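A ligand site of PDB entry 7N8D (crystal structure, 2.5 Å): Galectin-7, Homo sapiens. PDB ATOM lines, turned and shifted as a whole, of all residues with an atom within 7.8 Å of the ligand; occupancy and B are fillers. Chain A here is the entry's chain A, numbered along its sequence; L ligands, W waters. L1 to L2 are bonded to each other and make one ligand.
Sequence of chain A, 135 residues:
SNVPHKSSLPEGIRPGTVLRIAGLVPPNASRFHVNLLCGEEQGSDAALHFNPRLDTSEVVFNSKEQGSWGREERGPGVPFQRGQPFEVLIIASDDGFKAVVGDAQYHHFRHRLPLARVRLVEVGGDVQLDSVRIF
O3 of LIG L1 is in hydrogen-bond range of OE2 of Glu 72. An oxygen (O3) of LG2 L2 sits at hydrogen-bond distance from a ring nitrogen (NE2) of His 49 (2.9 Å). An oxygen (O3) of LIG L1 lies within hydrogen-bond range of the guanidinium group of Arg 53 (2.9 Å). O5 of LG2 L2 lies within hydrogen-bond range of ND2 of Asn 62 (3.2 Å). O3 of LG2 L2 is in hydrogen-bond range of OD1 of Asn 51 (3.5 Å).
NH2 of Arg 74 lies within salt-bridge range of OE1 of Glu 72, at 2.8 Å. O of Asn 62 lies within hydrogen-bond range of N of His 49, at 2.8 Å. A ring nitrogen (ND1) of His 49 is in hydrogen-bond range of the side-chain amide oxygen (OD1) of Asn 35. NE of Arg 53 sits at hydrogen-bond distance from OD1 of Asn 51 (2.8 Å). O of Gly 70 lies within hydrogen-bond range of ND2 of Asn 62 (2.7 Å). O of Arg 71 sits close to OD1 of Asn 62, 3.4 Å away. The backbone NH of Asn 51 lies within hydrogen-bond range of the backbone carbonyl oxygen of Val 60. The guanidinium group of Arg 74 lies within salt-bridge range of the side-chain carboxylate of Glu 58 (3.1 Å).
CG1 of Val 60 touches O5 of LG2 L2, 3.9 Å away. CE2 of Trp 69 touches C5 of LG2 L2, 3.7 Å away. NH1 of Arg 74 touches O3 of LIG L1 (3.999 Å). Hydrophobic or aromatic side chains within 4 Å of the ligand: His 49, Val 60 and Trp 69. The nearest printed residue that does not touch the ligand is Glu 58 (5.1 Å).
Water W2 lies within hydrogen-bond range of O2 of LG2 L2 and OD1 of Asn 51. Water W3 lies within hydrogen-bond range of NH2 of Arg 74 (3.1 Å) and O2 of LIG L1 (3.2 Å).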
ATOM      1  N   ARG A  31     -20.802  11.114   5.150  1.00  0.00           N
ATOM      2  CA  ARG A  31     -20.452  11.985   4.033  1.00  0.00           C
ATOM      3  C   ARG A  31     -18.994  12.389   4.137  1.00  0.00           C
ATOM      4  O   ARG A  31     -18.429  12.465   5.230  1.00  0.00           O
ATOM      5  CB  ARG A  31     -21.359  13.227   4.004  1.00  0.00           C
ATOM      6  CG  ARG A  31     -21.393  14.011   5.311  1.00  0.00           C
ATOM      7  CD  ARG A  31     -22.388  15.167   5.235  1.00  0.00           C
ATOM      8  NE  ARG A  31     -23.751  14.709   4.972  1.00  0.00           N
ATOM      9  CZ  ARG A  31     -24.795  15.508   4.830  1.00  0.00           C
ATOM     10  NH1 ARG A  31     -24.658  16.828   4.940  1.00  0.00           N
ATOM     11  NH2 ARG A  31     -25.994  15.005   4.585  1.00  0.00           N
ATOM     12  N   HIS A  33     -15.842  14.885   1.665  1.00  0.00           N
ATOM     13  CA  HIS A  33     -15.770  16.090   0.862  1.00  0.00           C
ATOM     14  C   HIS A  33     -14.370  16.294   0.303  1.00  0.00           C
ATOM     15  O   HIS A  33     -13.378  15.809   0.856  1.00  0.00           O
ATOM     16  CB  HIS A  33     -16.182  17.329   1.674  1.00  0.00           C
ATOM     17  CG  HIS A  33     -15.296  17.604   2.843  1.00  0.00           C
ATOM     18  ND1 HIS A  33     -15.597  17.186   4.123  1.00  0.00           N
ATOM     19  CD2 HIS A  33     -14.110  18.234   2.938  1.00  0.00           C
ATOM     20  CE1 HIS A  33     -14.640  17.554   4.954  1.00  0.00           C
ATOM     21  NE2 HIS A  33     -13.718  18.198   4.254  1.00  0.00           N
ATOM     22  N   ASN A  35     -12.305  19.780  -1.085  1.00  0.00           N
ATOM     23  CA  ASN A  35     -12.364  21.231  -1.181  1.00  0.00           C
ATOM     24  C   ASN A  35     -11.165  21.764  -1.956  1.00  0.00           C
ATOM     25  O   ASN A  35     -10.038  21.288  -1.787  1.00  0.00           O
ATOM     26  CB  ASN A  35     -12.401  21.895   0.202  1.00  0.00           C
ATOM     27  CG  ASN A  35     -13.673  21.596   0.963  1.00  0.00           C
ATOM     28  OD1 ASN A  35     -14.742  21.459   0.373  1.00  0.00           O
ATOM     29  ND2 ASN A  35     -13.563  21.514   2.289  1.00  0.00           N
ATOM     30  N   HIS A  49     -16.551  22.842  -3.883  1.00  0.00           N
ATOM     31  CA  HIS A  49     -16.886  22.030  -2.717  1.00  0.00           C
ATOM     32  C   HIS A  49     -17.628  20.803  -3.224  1.00  0.00           C
ATOM     33  O   HIS A  49     -18.757  20.907  -3.701  1.00  0.00           O
ATOM     34  CB  HIS A  49     -17.734  22.828  -1.720  1.00  0.00           C
ATOM     35  CG  HIS A  49     -18.360  22.000  -0.639  1.00  0.00           C
ATOM     36  ND1 HIS A  49     -17.621  21.348   0.326  1.00  0.00           N
ATOM     37  CD2 HIS A  49     -19.655  21.734  -0.365  1.00  0.00           C
ATOM     38  CE1 HIS A  49     -18.438  20.700   1.142  1.00  0.00           C
ATOM     39  NE2 HIS A  49     -19.682  20.928   0.739  1.00  0.00           N
ATOM     40  N   PHE A  50     -16.978  19.642  -3.130  1.00  0.00           N
ATOM     41  CA  PHE A  50     -17.458  18.387  -3.705  1.00  0.00           C
ATOM     42  C   PHE A  50     -17.797  17.462  -2.541  1.00  0.00           C
ATOM     43  O   PHE A  50     -16.894  17.004  -1.835  1.00  0.00           O
ATOM     44  CB  PHE A  50     -16.396  17.802  -4.637  1.00  0.00           C
ATOM     45  CG  PHE A  50     -16.701  16.408  -5.111  1.00  0.00           C
ATOM     46  CD1 PHE A  50     -17.602  16.187  -6.130  1.00  0.00           C
ATOM     47  CD2 PHE A  50     -16.034  15.325  -4.555  1.00  0.00           C
ATOM     48  CE1 PHE A  50     -17.866  14.903  -6.582  1.00  0.00           C
ATOM     49  CE2 PHE A  50     -16.289  14.042  -5.003  1.00  0.00           C
ATOM     50  CZ  PHE A  50     -17.203  13.833  -6.023  1.00  0.00           C
ATOM     51  N   ASN A  51     -19.086  17.193  -2.337  1.00  0.00           N
ATOM     52  CA  ASN A  51     -19.606  16.649  -1.085  1.00  0.00           C
ATOM     53  C   ASN A  51     -20.501  15.449  -1.336  1.00  0.00           C
ATOM     54  O   ASN A  51     -21.735  15.578  -1.382  1.00  0.00           O
ATOM     55  CB  ASN A  51     -20.353  17.743  -0.310  1.00  0.00           C
ATOM     56  CG  ASN A  51     -20.800  17.297   1.074  1.00  0.00           C
ATOM     57  OD1 ASN A  51     -21.887  17.635   1.520  1.00  0.00           O
ATOM     58  ND2 ASN A  51     -19.945  16.552   1.763  1.00  0.00           N
ATOM     59  N   ARG A  53     -22.709  12.563  -0.244  1.00  0.00           N
ATOM     60  CA  ARG A  53     -23.506  12.315   0.960  1.00  0.00           C
ATOM     61  C   ARG A  53     -24.149  10.947   0.849  1.00  0.00           C
ATOM     62  O   ARG A  53     -25.113  10.767   0.100  1.00  0.00           O
ATOM     63  CB  ARG A  53     -24.563  13.403   1.138  1.00  0.00           C
ATOM     64  CG  ARG A  53     -24.009  14.789   1.406  1.00  0.00           C
ATOM     65  CD  ARG A  53     -25.119  15.825   1.388  1.00  0.00           C
ATOM     66  NE  ARG A  53     -24.603  17.191   1.436  1.00  0.00           N
ATOM     67  CZ  ARG A  53     -25.367  18.276   1.489  1.00  0.00           C
ATOM     68  NH1 ARG A  53     -26.689  18.161   1.506  1.00  0.00           N
ATOM     69  NH2 ARG A  53     -24.804  19.481   1.536  1.00  0.00           N
ATOM     70  N   THR A  56     -27.817  10.858   2.843  1.00  0.00           N
ATOM     71  CA  THR A  56     -28.953  11.406   2.110  1.00  0.00           C
ATOM     72  C   THR A  56     -28.932  11.051   0.627  1.00  0.00           C
ATOM     73  O   THR A  56     -29.746  11.585  -0.138  1.00  0.00           O
ATOM     74  CB  THR A  56     -29.001  12.925   2.281  1.00  0.00           C
ATOM     75  OG1 THR A  56     -27.712  13.488   1.993  1.00  0.00           O
ATOM     76  CG2 THR A  56     -29.412  13.293   3.701  1.00  0.00           C
ATOM     77  N   GLU A  58     -27.001  11.577  -2.188  1.00  0.00           N
ATOM     78  CA  GLU A  58     -26.849  12.739  -3.064  1.00  0.00           C
ATOM     79  C   GLU A  58     -25.360  13.140  -3.141  1.00  0.00           C
ATOM     80  O   GLU A  58     -24.549  12.781  -2.274  1.00  0.00           O
ATOM     81  CB  GLU A  58     -27.713  13.920  -2.592  1.00  0.00           C
ATOM     82  CG  GLU A  58     -27.144  14.651  -1.405  1.00  0.00           C
ATOM     83  CD  GLU A  58     -28.153  15.539  -0.711  1.00  0.00           C
ATOM     84  OE1 GLU A  58     -29.250  15.922  -1.211  1.00  0.00           O
ATOM     85  OE2 GLU A  58     -27.863  15.905   0.412  1.00  0.00           O
ATOM     86  N   VAL A  60     -23.436  16.922  -3.791  1.00  0.00           N
ATOM     87  CA  VAL A  60     -23.691  18.349  -3.934  1.00  0.00           C
ATOM     88  C   VAL A  60     -22.409  19.053  -4.364  1.00  0.00           C
ATOM     89  O   VAL A  60     -21.329  18.788  -3.811  1.00  0.00           O
ATOM     90  CB  VAL A  60     -24.232  18.948  -2.628  1.00  0.00           C
ATOM     91  CG1 VAL A  60     -24.263  20.472  -2.687  1.00  0.00           C
ATOM     92  CG2 VAL A  60     -25.623  18.403  -2.338  1.00  0.00           C
ATOM     93  N   PHE A  61     -22.536  19.925  -5.357  1.00  0.00           N
ATOM     94  CA  PHE A  61     -21.477  20.821  -5.790  1.00  0.00           C
ATOM     95  C   PHE A  61     -21.855  22.240  -5.393  1.00  0.00           C
ATOM     96  O   PHE A  61     -23.013  22.632  -5.508  1.00  0.00           O
ATOM     97  CB  PHE A  61     -21.279  20.763  -7.310  1.00  0.00           C
ATOM     98  CG  PHE A  61     -20.799  19.434  -7.829  1.00  0.00           C
ATOM     99  CD1 PHE A  61     -21.582  18.302  -7.714  1.00  0.00           C
ATOM    100  CD2 PHE A  61     -19.580  19.335  -8.475  1.00  0.00           C
ATOM    101  CE1 PHE A  61     -21.152  17.081  -8.204  1.00  0.00           C
ATOM    102  CE2 PHE A  61     -19.136  18.119  -8.974  1.00  0.00           C
ATOM    103  CZ  PHE A  61     -19.926  16.996  -8.843  1.00  0.00           C
ATOM    104  N   ASN A  62     -20.869  23.018  -4.944  1.00  0.00           N
ATOM    105  CA  ASN A  62     -21.129  24.424  -4.668  1.00  0.00           C
ATOM    106  C   ASN A  62     -19.799  25.157  -4.507  1.00  0.00           C
ATOM    107  O   ASN A  62     -18.726  24.562  -4.535  1.00  0.00           O
ATOM    108  CB  ASN A  62     -21.989  24.590  -3.409  1.00  0.00           C
ATOM    109  CG  ASN A  62     -22.747  25.908  -3.406  1.00  0.00           C
ATOM    110  OD1 ASN A  62     -22.522  26.760  -4.264  1.00  0.00           O
ATOM    111  ND2 ASN A  62     -23.630  26.085  -2.438  1.00  0.00           N
ATOM    112  N   SER A  63     -19.912  26.472  -4.370  1.00  0.00           N
ATOM    113  CA  SER A  63     -18.784  27.356  -4.093  1.00  0.00           C
ATOM    114  C   SER A  63     -19.126  28.189  -2.878  1.00  0.00           C
ATOM    115  O   SER A  63     -20.285  28.282  -2.459  1.00  0.00           O
ATOM    116  CB  SER A  63     -18.483  28.266  -5.292  1.00  0.00           C
ATOM    117  OG  SER A  63     -19.629  29.030  -5.626  1.00  0.00           O
ATOM    118  N   LYS A  64     -18.107  28.829  -2.300  1.00  0.00           N
ATOM    119  CA  LYS A  64     -18.286  29.699  -1.149  1.00  0.00           C
ATOM    120  C   LYS A  64     -17.526  30.999  -1.378  1.00  0.00           C
ATOM    121  O   LYS A  64     -16.394  30.994  -1.871  1.00  0.00           O
ATOM    122  CB  LYS A  64     -17.810  29.036   0.139  1.00  0.00           C
ATOM    123  CG  LYS A  64     -18.252  29.781   1.389  1.00  0.00           C
ATOM    124  CD  LYS A  64     -18.642  28.843   2.522  1.00  0.00           C
ATOM    125  CE  LYS A  64     -17.465  28.512   3.419  1.00  0.00           C
ATOM    126  NZ  LYS A  64     -17.861  27.627   4.545  1.00  0.00           N
ATOM    127  N   TRP A  69     -22.719  30.525   0.828  1.00  0.00           N
ATOM    128  CA  TRP A  69     -22.726  29.527  -0.222  1.00  0.00           C
ATOM    129  C   TRP A  69     -23.435  30.052  -1.476  1.00  0.00           C
ATOM    130  O   TRP A  69     -24.386  30.839  -1.392  1.00  0.00           O
ATOM    131  CB  TRP A  69     -23.416  28.248   0.253  1.00  0.00           C
ATOM    132  CG  TRP A  69     -22.647  27.494   1.288  1.00  0.00           C
ATOM    133  CD1 TRP A  69     -22.907  27.441   2.627  1.00  0.00           C
ATOM    134  CD2 TRP A  69     -21.486  26.685   1.072  1.00  0.00           C
ATOM    135  NE1 TRP A  69     -21.985  26.639   3.255  1.00  0.00           N
ATOM    136  CE2 TRP A  69     -21.104  26.165   2.323  1.00  0.00           C
ATOM    137  CE3 TRP A  69     -20.739  26.342  -0.059  1.00  0.00           C
ATOM    138  CZ2 TRP A  69     -20.003  25.324   2.478  1.00  0.00           C
ATOM    139  CZ3 TRP A  69     -19.648  25.500   0.092  1.00  0.00           C
ATOM    140  CH2 TRP A  69     -19.295  25.009   1.350  1.00  0.00           C
ATOM    141  N   GLY A  70     -22.966  29.591  -2.631  1.00  0.00           N
ATOM    142  CA  GLY A  70     -23.650  29.849  -3.877  1.00  0.00           C
ATOM    143  C   GLY A  70     -24.764  28.847  -4.119  1.00  0.00           C
ATOM    144  O   GLY A  70     -25.174  28.093  -3.244  1.00  0.00           O
ATOM    145  N   ARG A  71     -25.259  28.850  -5.357  1.00  0.00           N
ATOM    146  CA  ARG A  71     -26.362  27.983  -5.730  1.00  0.00           C
ATOM    147  C   ARG A  71     -25.863  26.555  -5.913  1.00  0.00           C
ATOM    148  O   ARG A  71     -24.907  26.316  -6.663  1.00  0.00           O
ATOM    149  CB  ARG A  71     -27.020  28.478  -7.016  1.00  0.00           C
ATOM    150  CG  ARG A  71     -27.882  29.724  -6.814  1.00  0.00           C
ATOM    151  CD  ARG A  71     -28.101  30.465  -8.117  1.00  0.00           C
ATOM    152  NE  ARG A  71     -28.879  29.695  -9.075  1.00  0.00           N
ATOM    153  CZ  ARG A  71     -29.064  30.036 -10.343  1.00  0.00           C
ATOM    154  NH1 ARG A  71     -28.511  31.152 -10.823  1.00  0.00           N
ATOM    155  NH2 ARG A  71     -29.801  29.278 -11.139  1.00  0.00           N
ATOM    156  N   GLU A  72     -26.506  25.617  -5.227  1.00  0.00           N
ATOM    157  CA  GLU A  72     -26.069  24.227  -5.275  1.00  0.00           C
ATOM    158  C   GLU A  72     -26.325  23.614  -6.657  1.00  0.00           C
ATOM    159  O   GLU A  72     -27.267  23.972  -7.365  1.00  0.00           O
ATOM    160  CB  GLU A  72     -26.812  23.392  -4.224  1.00  0.00           C
ATOM    161  CG  GLU A  72     -26.408  23.684  -2.794  1.00  0.00           C
ATOM    162  CD  GLU A  72     -27.221  22.891  -1.800  1.00  0.00           C
ATOM    163  OE1 GLU A  72     -28.398  22.587  -2.092  1.00  0.00           O
ATOM    164  OE2 GLU A  72     -26.686  22.555  -0.722  1.00  0.00           O
ATOM    165  N   GLU A  73     -25.444  22.688  -7.023  1.00  0.00           N
ATOM    166  CA  GLU A  73     -25.675  21.779  -8.145  1.00  0.00           C
ATOM    167  C   GLU A  73     -25.573  20.349  -7.630  1.00  0.00           C
ATOM    168  O   GLU A  73     -24.727  20.044  -6.787  1.00  0.00           O
ATOM    169  CB  GLU A  73     -24.662  22.024  -9.264  1.00  0.00           C
ATOM    170  CG  GLU A  73     -24.710  23.417  -9.844  1.00  0.00           C
ATOM    171  CD  GLU A  73     -23.613  23.669 -10.851  1.00  0.00           C
ATOM    172  OE1 GLU A  73     -23.004  22.688 -11.334  1.00  0.00           O
ATOM    173  OE2 GLU A  73     -23.356  24.853 -11.167  1.00  0.00           O
ATOM    174  N   ARG A  74     -26.489  19.485  -8.085  1.00  0.00           N
ATOM    175  CA  ARG A  74     -26.558  18.064  -7.660  1.00  0.00           C
ATOM    176  C   ARG A  74     -26.336  17.204  -8.920  1.00  0.00           C
ATOM    177  O   ARG A  74     -26.827  17.577  -9.984  1.00  0.00           O
ATOM    178  CB  ARG A  74     -27.847  17.723  -6.872  1.00  0.00           C
ATOM    179  CG  ARG A  74     -27.618  17.187  -5.453  1.00  0.00           C
ATOM    180  CD  ARG A  74     -28.873  17.145  -4.538  1.00  0.00           C
ATOM    181  NE  ARG A  74     -29.417  18.509  -4.354  1.00  0.00           N
ATOM    182  CZ  ARG A  74     -29.324  19.313  -3.256  1.00  0.00           C
ATOM    183  NH1 ARG A  74     -28.754  18.889  -2.126  1.00  0.00           N
ATOM    184  NH2 ARG A  74     -29.861  20.536  -3.303  1.00  0.00           N
HETATM  185  C1  LIG L   1     -30.236  23.083   2.534  1.00  0.00           C
HETATM  186  C2  LIG L   1     -29.475  22.277   1.486  1.00  0.00           C
HETATM  187  C3  LIG L   1     -28.255  21.708   2.099  1.00  0.00           C
HETATM  188  C4  LIG L   1     -27.332  22.782   2.592  1.00  0.00           C
HETATM  189  C5  LIG L   1     -28.029  23.829   3.479  1.00  0.00           C
HETATM  190  C6  LIG L   1     -27.242  25.119   3.454  1.00  0.00           C
HETATM  191  O1  LIG L   1     -30.588  22.267   3.558  1.00  0.00           O
HETATM  192  O2  LIG L   1     -30.320  21.217   1.010  1.00  0.00           O
HETATM  193  O3  LIG L   1     -27.549  20.928   1.096  1.00  0.00           O
HETATM  194  O4  LIG L   1     -26.326  22.098   3.372  1.00  0.00           O
HETATM  195  O5  LIG L   1     -29.402  24.216   3.064  1.00  0.00           O
HETATM  196  O6  LIG L   1     -28.093  26.152   3.021  1.00  0.00           O
HETATM  197  C1  LG2 L   2     -25.096  22.652   3.258  1.00  0.00           C
HETATM  198  C2  LG2 L   2     -24.111  21.846   4.105  1.00  0.00           C
HETATM  199  C3  LG2 L   2     -22.731  22.375   3.980  1.00  0.00           C
HETATM  200  C4  LG2 L   2     -22.302  22.396   2.532  1.00  0.00           C
HETATM  201  C5  LG2 L   2     -23.289  23.225   1.708  1.00  0.00           C
HETATM  202  C6  LG2 L   2     -22.904  23.258   0.256  1.00  0.00           C
HETATM  203  O1  LG2 L   2     -24.545  21.912   5.480  1.00  0.00           O
HETATM  204  O2  LG2 L   2     -21.835  21.540   4.762  1.00  0.00           O
HETATM  205  O3  LG2 L   2     -22.248  21.045   2.075  1.00  0.00           O
HETATM  206  O4  LG2 L   2     -24.662  22.679   1.822  1.00  0.00           O
HETATM  207  O5  LG2 L   2     -24.024  23.645  -0.481  1.00  0.00           O
HETATM  208  O   HOH W   1     -32.452  19.445   1.190  1.00  0.00           O
HETATM  209  O   HOH W   2     -21.520  18.654   4.632  1.00  0.00           O
HETATM  210  O   HOH W   3     -31.951  22.033  -1.587  1.00  0.00           O
